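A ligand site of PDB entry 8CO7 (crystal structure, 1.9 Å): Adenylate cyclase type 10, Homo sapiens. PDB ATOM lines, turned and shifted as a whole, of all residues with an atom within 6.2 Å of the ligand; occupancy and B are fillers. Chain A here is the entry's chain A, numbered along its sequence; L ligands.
Phe 45 touches the ligand (CE1 to C7, 3.7 Å).
Lys 95 touches the ligand (O to C13, 3.5 Å).
Phe 96 touches the ligand (C to C13, 3.7 Å).
N of Ala 97 touches C13 of the ligand, 3.4 Å away.
O of Ala 100 touches C13 of the ligand, 3.9 Å away.
Leu 101 touches the ligand (CA to C13, 3.9 Å).
Leu 102 touches the ligand (CD2 to C10, 3.5 Å).
Phe 165 touches the ligand (CE2 to CL1, 3.3 Å).
CA of Leu 166 touches N3 of the ligand, at 3.8 Å.
Val 172 touches the ligand (O to C3, 3.4 Å).
Val 175 touches the ligand (CG1 to C2, 3.8 Å).
Arg 176 touches the ligand (CG to C2, 3.5 Å).
CD1 of Phe 336 touches C6 of the ligand, 3.3 Å away.
15 residues have an atom within 4 Å of the ligand: Phe 45, Lys 95, Phe 96, Ala 97, Ala 100, Leu 101, Leu 102, Phe 165, Leu 166, Val 167, Val 172, Val 175, Arg 176, Phe 336 and Met 337.
O of Met 337 is in hydrogen-bond range of N5 of the ligand (2.6 Å).
A nitrogen (N3) of the ligand lies within hydrogen-bond range of the backbone NH of Val 167.
The backbone carbonyl oxygen (O) of Val 167 is in hydrogen-bond range of a nitrogen (N5) of the ligand (2.8 Å).
NZ of Lys 95 is in hydrogen-bond range of O of Phe 165 (2.9 Å).
The backbone NH of Leu 102 is in hydrogen-bond range of the backbone carbonyl oxygen of Lys 95, at 3.1 Å.
The backbone carbonyl oxygen of Leu 102 lies within hydrogen-bond range of the backbone NH of Leu 94, 2.7 Å away.
The side-chain amino group (NZ) of Lys 95 sits at hydrogen-bond distance from the backbone carbonyl oxygen (O) of Val 335.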
ATOM      1  N   LEU A  23       9.626  16.823  22.197  1.00  0.00           N
ATOM      2  CA  LEU A  23      10.835  16.734  21.381  1.00  0.00           C
ATOM      3  C   LEU A  23      11.152  15.288  20.997  1.00  0.00           C
ATOM      4  O   LEU A  23      11.601  15.017  19.873  1.00  0.00           O
ATOM      5  CB  LEU A  23      12.025  17.310  22.136  1.00  0.00           C
ATOM      6  CG  LEU A  23      13.358  17.410  21.396  1.00  0.00           C
ATOM      7  CD1 LEU A  23      13.226  18.395  20.230  1.00  0.00           C
ATOM      8  CD2 LEU A  23      14.433  17.870  22.317  1.00  0.00           C
ATOM      9  N   LEU A  43      14.591  28.942  25.654  1.00  0.00           N
ATOM     10  CA  LEU A  43      14.766  28.018  26.767  1.00  0.00           C
ATOM     11  C   LEU A  43      14.468  28.759  28.061  1.00  0.00           C
ATOM     12  O   LEU A  43      14.743  29.947  28.178  1.00  0.00           O
ATOM     13  CB  LEU A  43      16.182  27.447  26.822  1.00  0.00           C
ATOM     14  CG  LEU A  43      16.538  26.567  25.612  1.00  0.00           C
ATOM     15  CD1 LEU A  43      18.026  26.403  25.572  1.00  0.00           C
ATOM     16  CD2 LEU A  43      15.859  25.267  25.695  1.00  0.00           C
ATOM     17  N   PHE A  45      15.252  27.960  32.161  1.00  0.00           N
ATOM     18  CA  PHE A  45      15.787  27.140  33.258  1.00  0.00           C
ATOM     19  C   PHE A  45      15.297  27.722  34.576  1.00  0.00           C
ATOM     20  O   PHE A  45      15.398  28.940  34.793  1.00  0.00           O
ATOM     21  CB  PHE A  45      17.320  27.099  33.227  1.00  0.00           C
ATOM     22  CG  PHE A  45      17.902  26.074  34.184  1.00  0.00           C
ATOM     23  CD1 PHE A  45      17.439  24.764  34.185  1.00  0.00           C
ATOM     24  CD2 PHE A  45      18.870  26.432  35.082  1.00  0.00           C
ATOM     25  CE1 PHE A  45      17.954  23.841  35.062  1.00  0.00           C
ATOM     26  CE2 PHE A  45      19.396  25.504  35.984  1.00  0.00           C
ATOM     27  CZ  PHE A  45      18.956  24.229  35.983  1.00  0.00           C
ATOM     28  N   LEU A  94      11.938  19.578  29.047  1.00  0.00           N
ATOM     29  CA  LEU A  94      12.884  18.636  28.455  1.00  0.00           C
ATOM     30  C   LEU A  94      13.364  17.628  29.493  1.00  0.00           C
ATOM     31  O   LEU A  94      13.353  16.419  29.239  1.00  0.00           O
ATOM     32  CB  LEU A  94      14.063  19.365  27.843  1.00  0.00           C
ATOM     33  CG  LEU A  94      13.821  20.331  26.706  1.00  0.00           C
ATOM     34  CD1 LEU A  94      15.165  20.854  26.163  1.00  0.00           C
ATOM     35  CD2 LEU A  94      13.015  19.645  25.558  1.00  0.00           C
ATOM     36  N   LYS A  95      13.763  18.094  30.668  1.00  0.00           N
ATOM     37  CA  LYS A  95      14.303  17.238  31.715  1.00  0.00           C
ATOM     38  C   LYS A  95      14.092  17.884  33.090  1.00  0.00           C
ATOM     39  O   LYS A  95      14.007  19.120  33.204  1.00  0.00           O
ATOM     40  CB  LYS A  95      15.820  16.980  31.521  1.00  0.00           C
ATOM     41  CG  LYS A  95      16.140  15.856  30.571  1.00  0.00           C
ATOM     42  CD  LYS A  95      17.646  15.462  30.627  1.00  0.00           C
ATOM     43  CE  LYS A  95      17.961  14.532  29.456  1.00  0.00           C
ATOM     44  NZ  LYS A  95      19.390  14.227  29.337  1.00  0.00           N
ATOM     45  N   PHE A  96      13.997  17.026  34.094  1.00  0.00           N
ATOM     46  CA  PHE A  96      14.018  17.405  35.493  1.00  0.00           C
ATOM     47  C   PHE A  96      15.312  16.914  36.143  1.00  0.00           C
ATOM     48  O   PHE A  96      15.827  15.844  35.798  1.00  0.00           O
ATOM     49  CB  PHE A  96      12.874  16.791  36.322  1.00  0.00           C
ATOM     50  CG  PHE A  96      11.499  17.132  35.856  1.00  0.00           C
ATOM     51  CD1 PHE A  96      10.940  16.462  34.792  1.00  0.00           C
ATOM     52  CD2 PHE A  96      10.755  18.068  36.546  1.00  0.00           C
ATOM     53  CE1 PHE A  96       9.642  16.760  34.384  1.00  0.00           C
ATOM     54  CE2 PHE A  96       9.462  18.367  36.160  1.00  0.00           C
ATOM     55  CZ  PHE A  96       8.912  17.679  35.072  1.00  0.00           C
ATOM     56  N   ALA A  97      15.793  17.692  37.100  1.00  0.00           N
ATOM     57  CA  ALA A  97      16.870  17.289  37.984  1.00  0.00           C
ATOM     58  C   ALA A  97      16.560  17.873  39.341  1.00  0.00           C
ATOM     59  O   ALA A  97      16.499  19.090  39.487  1.00  0.00           O
ATOM     60  CB  ALA A  97      18.236  17.766  37.484  1.00  0.00           C
ATOM     61  N   ALA A 100      15.011  21.375  39.787  1.00  0.00           N
ATOM     62  CA  ALA A 100      15.268  22.212  38.612  1.00  0.00           C
ATOM     63  C   ALA A 100      14.634  21.572  37.398  1.00  0.00           C
ATOM     64  O   ALA A 100      14.404  20.356  37.374  1.00  0.00           O
ATOM     65  CB  ALA A 100      16.780  22.390  38.380  1.00  0.00           C
ATOM     66  N   LEU A 101      14.323  22.389  36.391  1.00  0.00           N
ATOM     67  CA  LEU A 101      13.847  21.848  35.131  1.00  0.00           C
ATOM     68  C   LEU A 101      14.195  22.794  33.996  1.00  0.00           C
ATOM     69  O   LEU A 101      14.279  24.008  34.180  1.00  0.00           O
ATOM     70  CB  LEU A 101      12.321  21.561  35.145  1.00  0.00           C
ATOM     71  CG  LEU A 101      11.333  22.732  35.160  1.00  0.00           C
ATOM     72  CD1 LEU A 101      11.086  23.341  33.800  1.00  0.00           C
ATOM     73  CD2 LEU A 101       9.985  22.245  35.753  1.00  0.00           C
ATOM     74  N   LEU A 102      14.385  22.215  32.820  1.00  0.00           N
ATOM     75  CA  LEU A 102      14.708  22.928  31.595  1.00  0.00           C
ATOM     76  C   LEU A 102      13.546  22.780  30.635  1.00  0.00           C
ATOM     77  O   LEU A 102      13.086  21.654  30.409  1.00  0.00           O
ATOM     78  CB  LEU A 102      15.984  22.368  30.947  1.00  0.00           C
ATOM     79  CG  LEU A 102      16.447  23.078  29.683  1.00  0.00           C
ATOM     80  CD1 LEU A 102      16.939  24.482  30.015  1.00  0.00           C
ATOM     81  CD2 LEU A 102      17.573  22.252  28.975  1.00  0.00           C
ATOM     82  N   PHE A 165      19.116  11.729  25.339  1.00  0.00           N
ATOM     83  CA  PHE A 165      19.089  12.917  24.491  1.00  0.00           C
ATOM     84  C   PHE A 165      19.591  14.133  25.249  1.00  0.00           C
ATOM     85  O   PHE A 165      19.559  14.178  26.476  1.00  0.00           O
ATOM     86  CB  PHE A 165      17.681  13.222  23.928  1.00  0.00           C
ATOM     87  CG  PHE A 165      16.710  13.766  24.951  1.00  0.00           C
ATOM     88  CD1 PHE A 165      15.992  12.923  25.743  1.00  0.00           C
ATOM     89  CD2 PHE A 165      16.552  15.134  25.112  1.00  0.00           C
ATOM     90  CE1 PHE A 165      15.105  13.412  26.700  1.00  0.00           C
ATOM     91  CE2 PHE A 165      15.669  15.624  26.036  1.00  0.00           C
ATOM     92  CZ  PHE A 165      14.951  14.777  26.819  1.00  0.00           C
ATOM     93  N   LEU A 166      20.104  15.101  24.482  1.00  0.00           N
ATOM     94  CA  LEU A 166      20.580  16.369  24.988  1.00  0.00           C
ATOM     95  C   LEU A 166      20.223  17.469  24.011  1.00  0.00           C
ATOM     96  O   LEU A 166      19.974  17.218  22.829  1.00  0.00           O
ATOM     97  CB  LEU A 166      22.098  16.374  25.164  1.00  0.00           C
ATOM     98  CG  LEU A 166      22.708  15.432  26.199  1.00  0.00           C
ATOM     99  CD1 LEU A 166      24.153  15.333  25.932  1.00  0.00           C
ATOM    100  CD2 LEU A 166      22.437  15.980  27.586  1.00  0.00           C
ATOM    101  N   VAL A 167      20.221  18.720  24.519  1.00  0.00           N
ATOM    102  CA  VAL A 167      20.271  19.900  23.682  1.00  0.00           C
ATOM    103  C   VAL A 167      21.606  20.586  23.940  1.00  0.00           C
ATOM    104  O   VAL A 167      22.132  20.538  25.056  1.00  0.00           O
ATOM    105  CB  VAL A 167      19.097  20.880  23.908  1.00  0.00           C
ATOM    106  CG1 VAL A 167      17.854  20.317  23.251  1.00  0.00           C
ATOM    107  CG2 VAL A 167      18.851  21.153  25.378  1.00  0.00           C
ATOM    108  N   ILE A 168      22.153  21.217  22.912  1.00  0.00           N
ATOM    109  CA  ILE A 168      23.529  21.712  22.894  1.00  0.00           C
ATOM    110  C   ILE A 168      23.562  23.059  22.183  1.00  0.00           C
ATOM    111  O   ILE A 168      22.751  23.306  21.303  1.00  0.00           O
ATOM    112  CB  ILE A 168      24.474  20.718  22.172  1.00  0.00           C
ATOM    113  CG1 ILE A 168      24.608  19.428  22.997  1.00  0.00           C
ATOM    114  CG2 ILE A 168      25.813  21.289  21.935  1.00  0.00           C
ATOM    115  CD1 ILE A 168      25.292  18.304  22.226  1.00  0.00           C
ATOM    116  N   ALA A 171      22.850  28.982  23.046  1.00  0.00           N
ATOM    117  CA  ALA A 171      21.597  29.277  23.741  1.00  0.00           C
ATOM    118  C   ALA A 171      21.451  28.409  24.994  1.00  0.00           C
ATOM    119  O   ALA A 171      20.968  28.889  26.039  1.00  0.00           O
ATOM    120  CB  ALA A 171      20.402  29.081  22.808  1.00  0.00           C
ATOM    121  N   VAL A 172      21.853  27.141  24.915  1.00  0.00           N
ATOM    122  CA  VAL A 172      21.837  26.285  26.089  1.00  0.00           C
ATOM    123  C   VAL A 172      22.830  26.813  27.126  1.00  0.00           C
ATOM    124  O   VAL A 172      22.515  26.989  28.302  1.00  0.00           O
ATOM    125  CB  VAL A 172      22.134  24.829  25.696  1.00  0.00           C
ATOM    126  CG1 VAL A 172      22.212  23.956  26.920  1.00  0.00           C
ATOM    127  CG2 VAL A 172      21.065  24.279  24.759  1.00  0.00           C
ATOM    128  N   ASP A 173      24.068  27.067  26.693  1.00  0.00           N
ATOM    129  CA  ASP A 173      25.038  27.621  27.619  1.00  0.00           C
ATOM    130  C   ASP A 173      24.532  28.935  28.190  1.00  0.00           C
ATOM    131  O   ASP A 173      24.731  29.201  29.382  1.00  0.00           O
ATOM    132  CB  ASP A 173      26.378  27.833  26.910  1.00  0.00           C
ATOM    133  CG  ASP A 173      26.966  26.528  26.376  1.00  0.00           C
ATOM    134  OD1 ASP A 173      26.530  25.454  26.816  1.00  0.00           O
ATOM    135  OD2 ASP A 173      27.883  26.618  25.533  1.00  0.00           O
ATOM    136  N   VAL A 175      21.436  30.082  28.768  1.00  0.00           N
ATOM    137  CA  VAL A 175      20.367  29.994  29.758  1.00  0.00           C
ATOM    138  C   VAL A 175      20.899  29.478  31.078  1.00  0.00           C
ATOM    139  O   VAL A 175      20.441  29.900  32.139  1.00  0.00           O
ATOM    140  CB  VAL A 175      19.192  29.138  29.239  1.00  0.00           C
ATOM    141  CG1 VAL A 175      19.449  27.660  29.372  1.00  0.00           C
ATOM    142  CG2 VAL A 175      17.921  29.482  29.977  1.00  0.00           C
ATOM    143  N   ARG A 176      21.898  28.602  31.040  1.00  0.00           N
ATOM    144  CA  ARG A 176      22.541  28.169  32.283  1.00  0.00           C
ATOM    145  C   ARG A 176      23.176  29.355  32.992  1.00  0.00           C
ATOM    146  O   ARG A 176      23.000  29.534  34.203  1.00  0.00           O
ATOM    147  CB  ARG A 176      23.592  27.093  31.986  1.00  0.00           C
ATOM    148  CG  ARG A 176      23.751  26.042  33.085  1.00  0.00           C
ATOM    149  CD  ARG A 176      24.550  26.585  34.258  1.00  0.00           C
ATOM    150  NE  ARG A 176      25.835  27.160  33.872  1.00  0.00           N
ATOM    151  CZ  ARG A 176      26.684  27.712  34.732  1.00  0.00           C
ATOM    152  NH1 ARG A 176      27.829  28.220  34.305  1.00  0.00           N
ATOM    153  NH2 ARG A 176      26.382  27.762  36.016  1.00  0.00           N
ATOM    154  N   LEU A 177      23.911  30.176  32.242  1.00  0.00           N
ATOM    155  CA  LEU A 177      24.579  31.322  32.840  1.00  0.00           C
ATOM    156  C   LEU A 177      23.582  32.361  33.342  1.00  0.00           C
ATOM    157  O   LEU A 177      23.734  32.893  34.443  1.00  0.00           O
ATOM    158  CB  LEU A 177      25.532  31.947  31.813  1.00  0.00           C
ATOM    159  CG  LEU A 177      26.857  31.211  31.632  1.00  0.00           C
ATOM    160  CD1 LEU A 177      27.443  31.454  30.236  1.00  0.00           C
ATOM    161  CD2 LEU A 177      27.864  31.636  32.702  1.00  0.00           C
ATOM    162  N   VAL A 335      21.818  12.721  32.094  1.00  0.00           N
ATOM    163  CA  VAL A 335      22.914  13.223  31.284  1.00  0.00           C
ATOM    164  C   VAL A 335      22.597  14.689  30.976  1.00  0.00           C
ATOM    165  O   VAL A 335      21.457  15.008  30.630  1.00  0.00           O
ATOM    166  CB  VAL A 335      23.084  12.426  29.978  1.00  0.00           C
ATOM    167  CG1 VAL A 335      24.385  12.843  29.279  1.00  0.00           C
ATOM    168  CG2 VAL A 335      23.054  10.916  30.247  1.00  0.00           C
ATOM    169  N   PHE A 336      23.602  15.557  31.115  1.00  0.00           N
ATOM    170  CA  PHE A 336      23.477  16.992  30.937  1.00  0.00           C
ATOM    171  C   PHE A 336      24.680  17.478  30.123  1.00  0.00           C
ATOM    172  O   PHE A 336      25.692  16.785  30.067  1.00  0.00           O
ATOM    173  CB  PHE A 336      23.477  17.798  32.256  1.00  0.00           C
ATOM    174  CG  PHE A 336      22.598  17.240  33.329  1.00  0.00           C
ATOM    175  CD1 PHE A 336      21.225  17.454  33.306  1.00  0.00           C
ATOM    176  CD2 PHE A 336      23.141  16.558  34.391  1.00  0.00           C
ATOM    177  CE1 PHE A 336      20.375  16.960  34.333  1.00  0.00           C
ATOM    178  CE2 PHE A 336      22.314  16.066  35.409  1.00  0.00           C
ATOM    179  CZ  PHE A 336      20.923  16.313  35.371  1.00  0.00           C
ATOM    180  N   MET A 337      24.563  18.682  29.563  1.00  0.00           N
ATOM    181  CA  MET A 337      25.677  19.310  28.878  1.00  0.00           C
ATOM    182  C   MET A 337      25.574  20.823  28.898  1.00  0.00           C
ATOM    183  O   MET A 337      24.543  21.398  28.524  1.00  0.00           O
ATOM    184  CB  MET A 337      25.753  18.862  27.419  1.00  0.00           C
ATOM    185  CG  MET A 337      27.043  19.292  26.767  1.00  0.00           C
ATOM    186  SD  MET A 337      27.245  18.372  25.276  1.00  0.00           S
ATOM    187  CE  MET A 337      28.862  18.267  24.932  1.00  0.00           C
ATOM    188  N   PHE A 338      26.688  21.475  29.278  1.00  0.00           N
ATOM    189  CA  PHE A 338      26.808  22.913  29.134  1.00  0.00           C
ATOM    190  C   PHE A 338      28.273  23.290  29.294  1.00  0.00           C
ATOM    191  O   PHE A 338      29.053  22.593  29.964  1.00  0.00           O
ATOM    192  CB  PHE A 338      25.907  23.655  30.149  1.00  0.00           C
ATOM    193  CG  PHE A 338      26.146  23.283  31.585  1.00  0.00           C
ATOM    194  CD1 PHE A 338      27.133  23.922  32.326  1.00  0.00           C
ATOM    195  CD2 PHE A 338      25.349  22.350  32.233  1.00  0.00           C
ATOM    196  CE1 PHE A 338      27.321  23.611  33.657  1.00  0.00           C
ATOM    197  CE2 PHE A 338      25.545  22.041  33.553  1.00  0.00           C
ATOM    198  CZ  PHE A 338      26.550  22.681  34.262  1.00  0.00           C
HETATM  199  C1  LIG L   1      20.724  23.681  32.590  1.00  0.00           C
HETATM  200  C2  LIG L   1      20.760  24.904  31.571  1.00  0.00           C
HETATM  201  C3  LIG L   1      21.353  24.459  30.327  1.00  0.00           C
HETATM  202  C4  LIG L   1      21.308  22.552  31.941  1.00  0.00           C
HETATM  203  C5  LIG L   1      19.332  19.897  31.892  1.00  0.00           C
HETATM  204  C6  LIG L   1      20.087  20.560  32.805  1.00  0.00           C
HETATM  205  C7  LIG L   1      19.367  20.604  33.940  1.00  0.00           C
HETATM  206  C8  LIG L   1      21.185  19.678  28.460  1.00  0.00           C
HETATM  207  C9  LIG L   1      19.675  19.595  30.444  1.00  0.00           C
HETATM  208  C10 LIG L   1      18.646  18.938  29.631  1.00  0.00           C
HETATM  209  C11 LIG L   1      18.925  18.647  28.237  1.00  0.00           C
HETATM  210  C12 LIG L   1      21.478  21.158  32.551  1.00  0.00           C
HETATM  211  C13 LIG L   1      17.145  19.743  34.737  1.00  0.00           C
HETATM  212  N1  LIG L   1      18.232  19.955  33.753  1.00  0.00           N
HETATM  213  N2  LIG L   1      18.183  19.545  32.461  1.00  0.00           N
HETATM  214  N3  LIG L   1      20.177  18.997  27.647  1.00  0.00           N
HETATM  215  N4  LIG L   1      20.923  19.974  29.831  1.00  0.00           N
HETATM  216  N5  LIG L   1      22.407  20.068  27.828  1.00  0.00           N
HETATM  217  S1  LIG L   1      21.749  22.968  30.491  1.00  0.00           S
HETATM  218 CL1  LIG L   1      17.760  17.824  27.271  1.00  0.00          CL
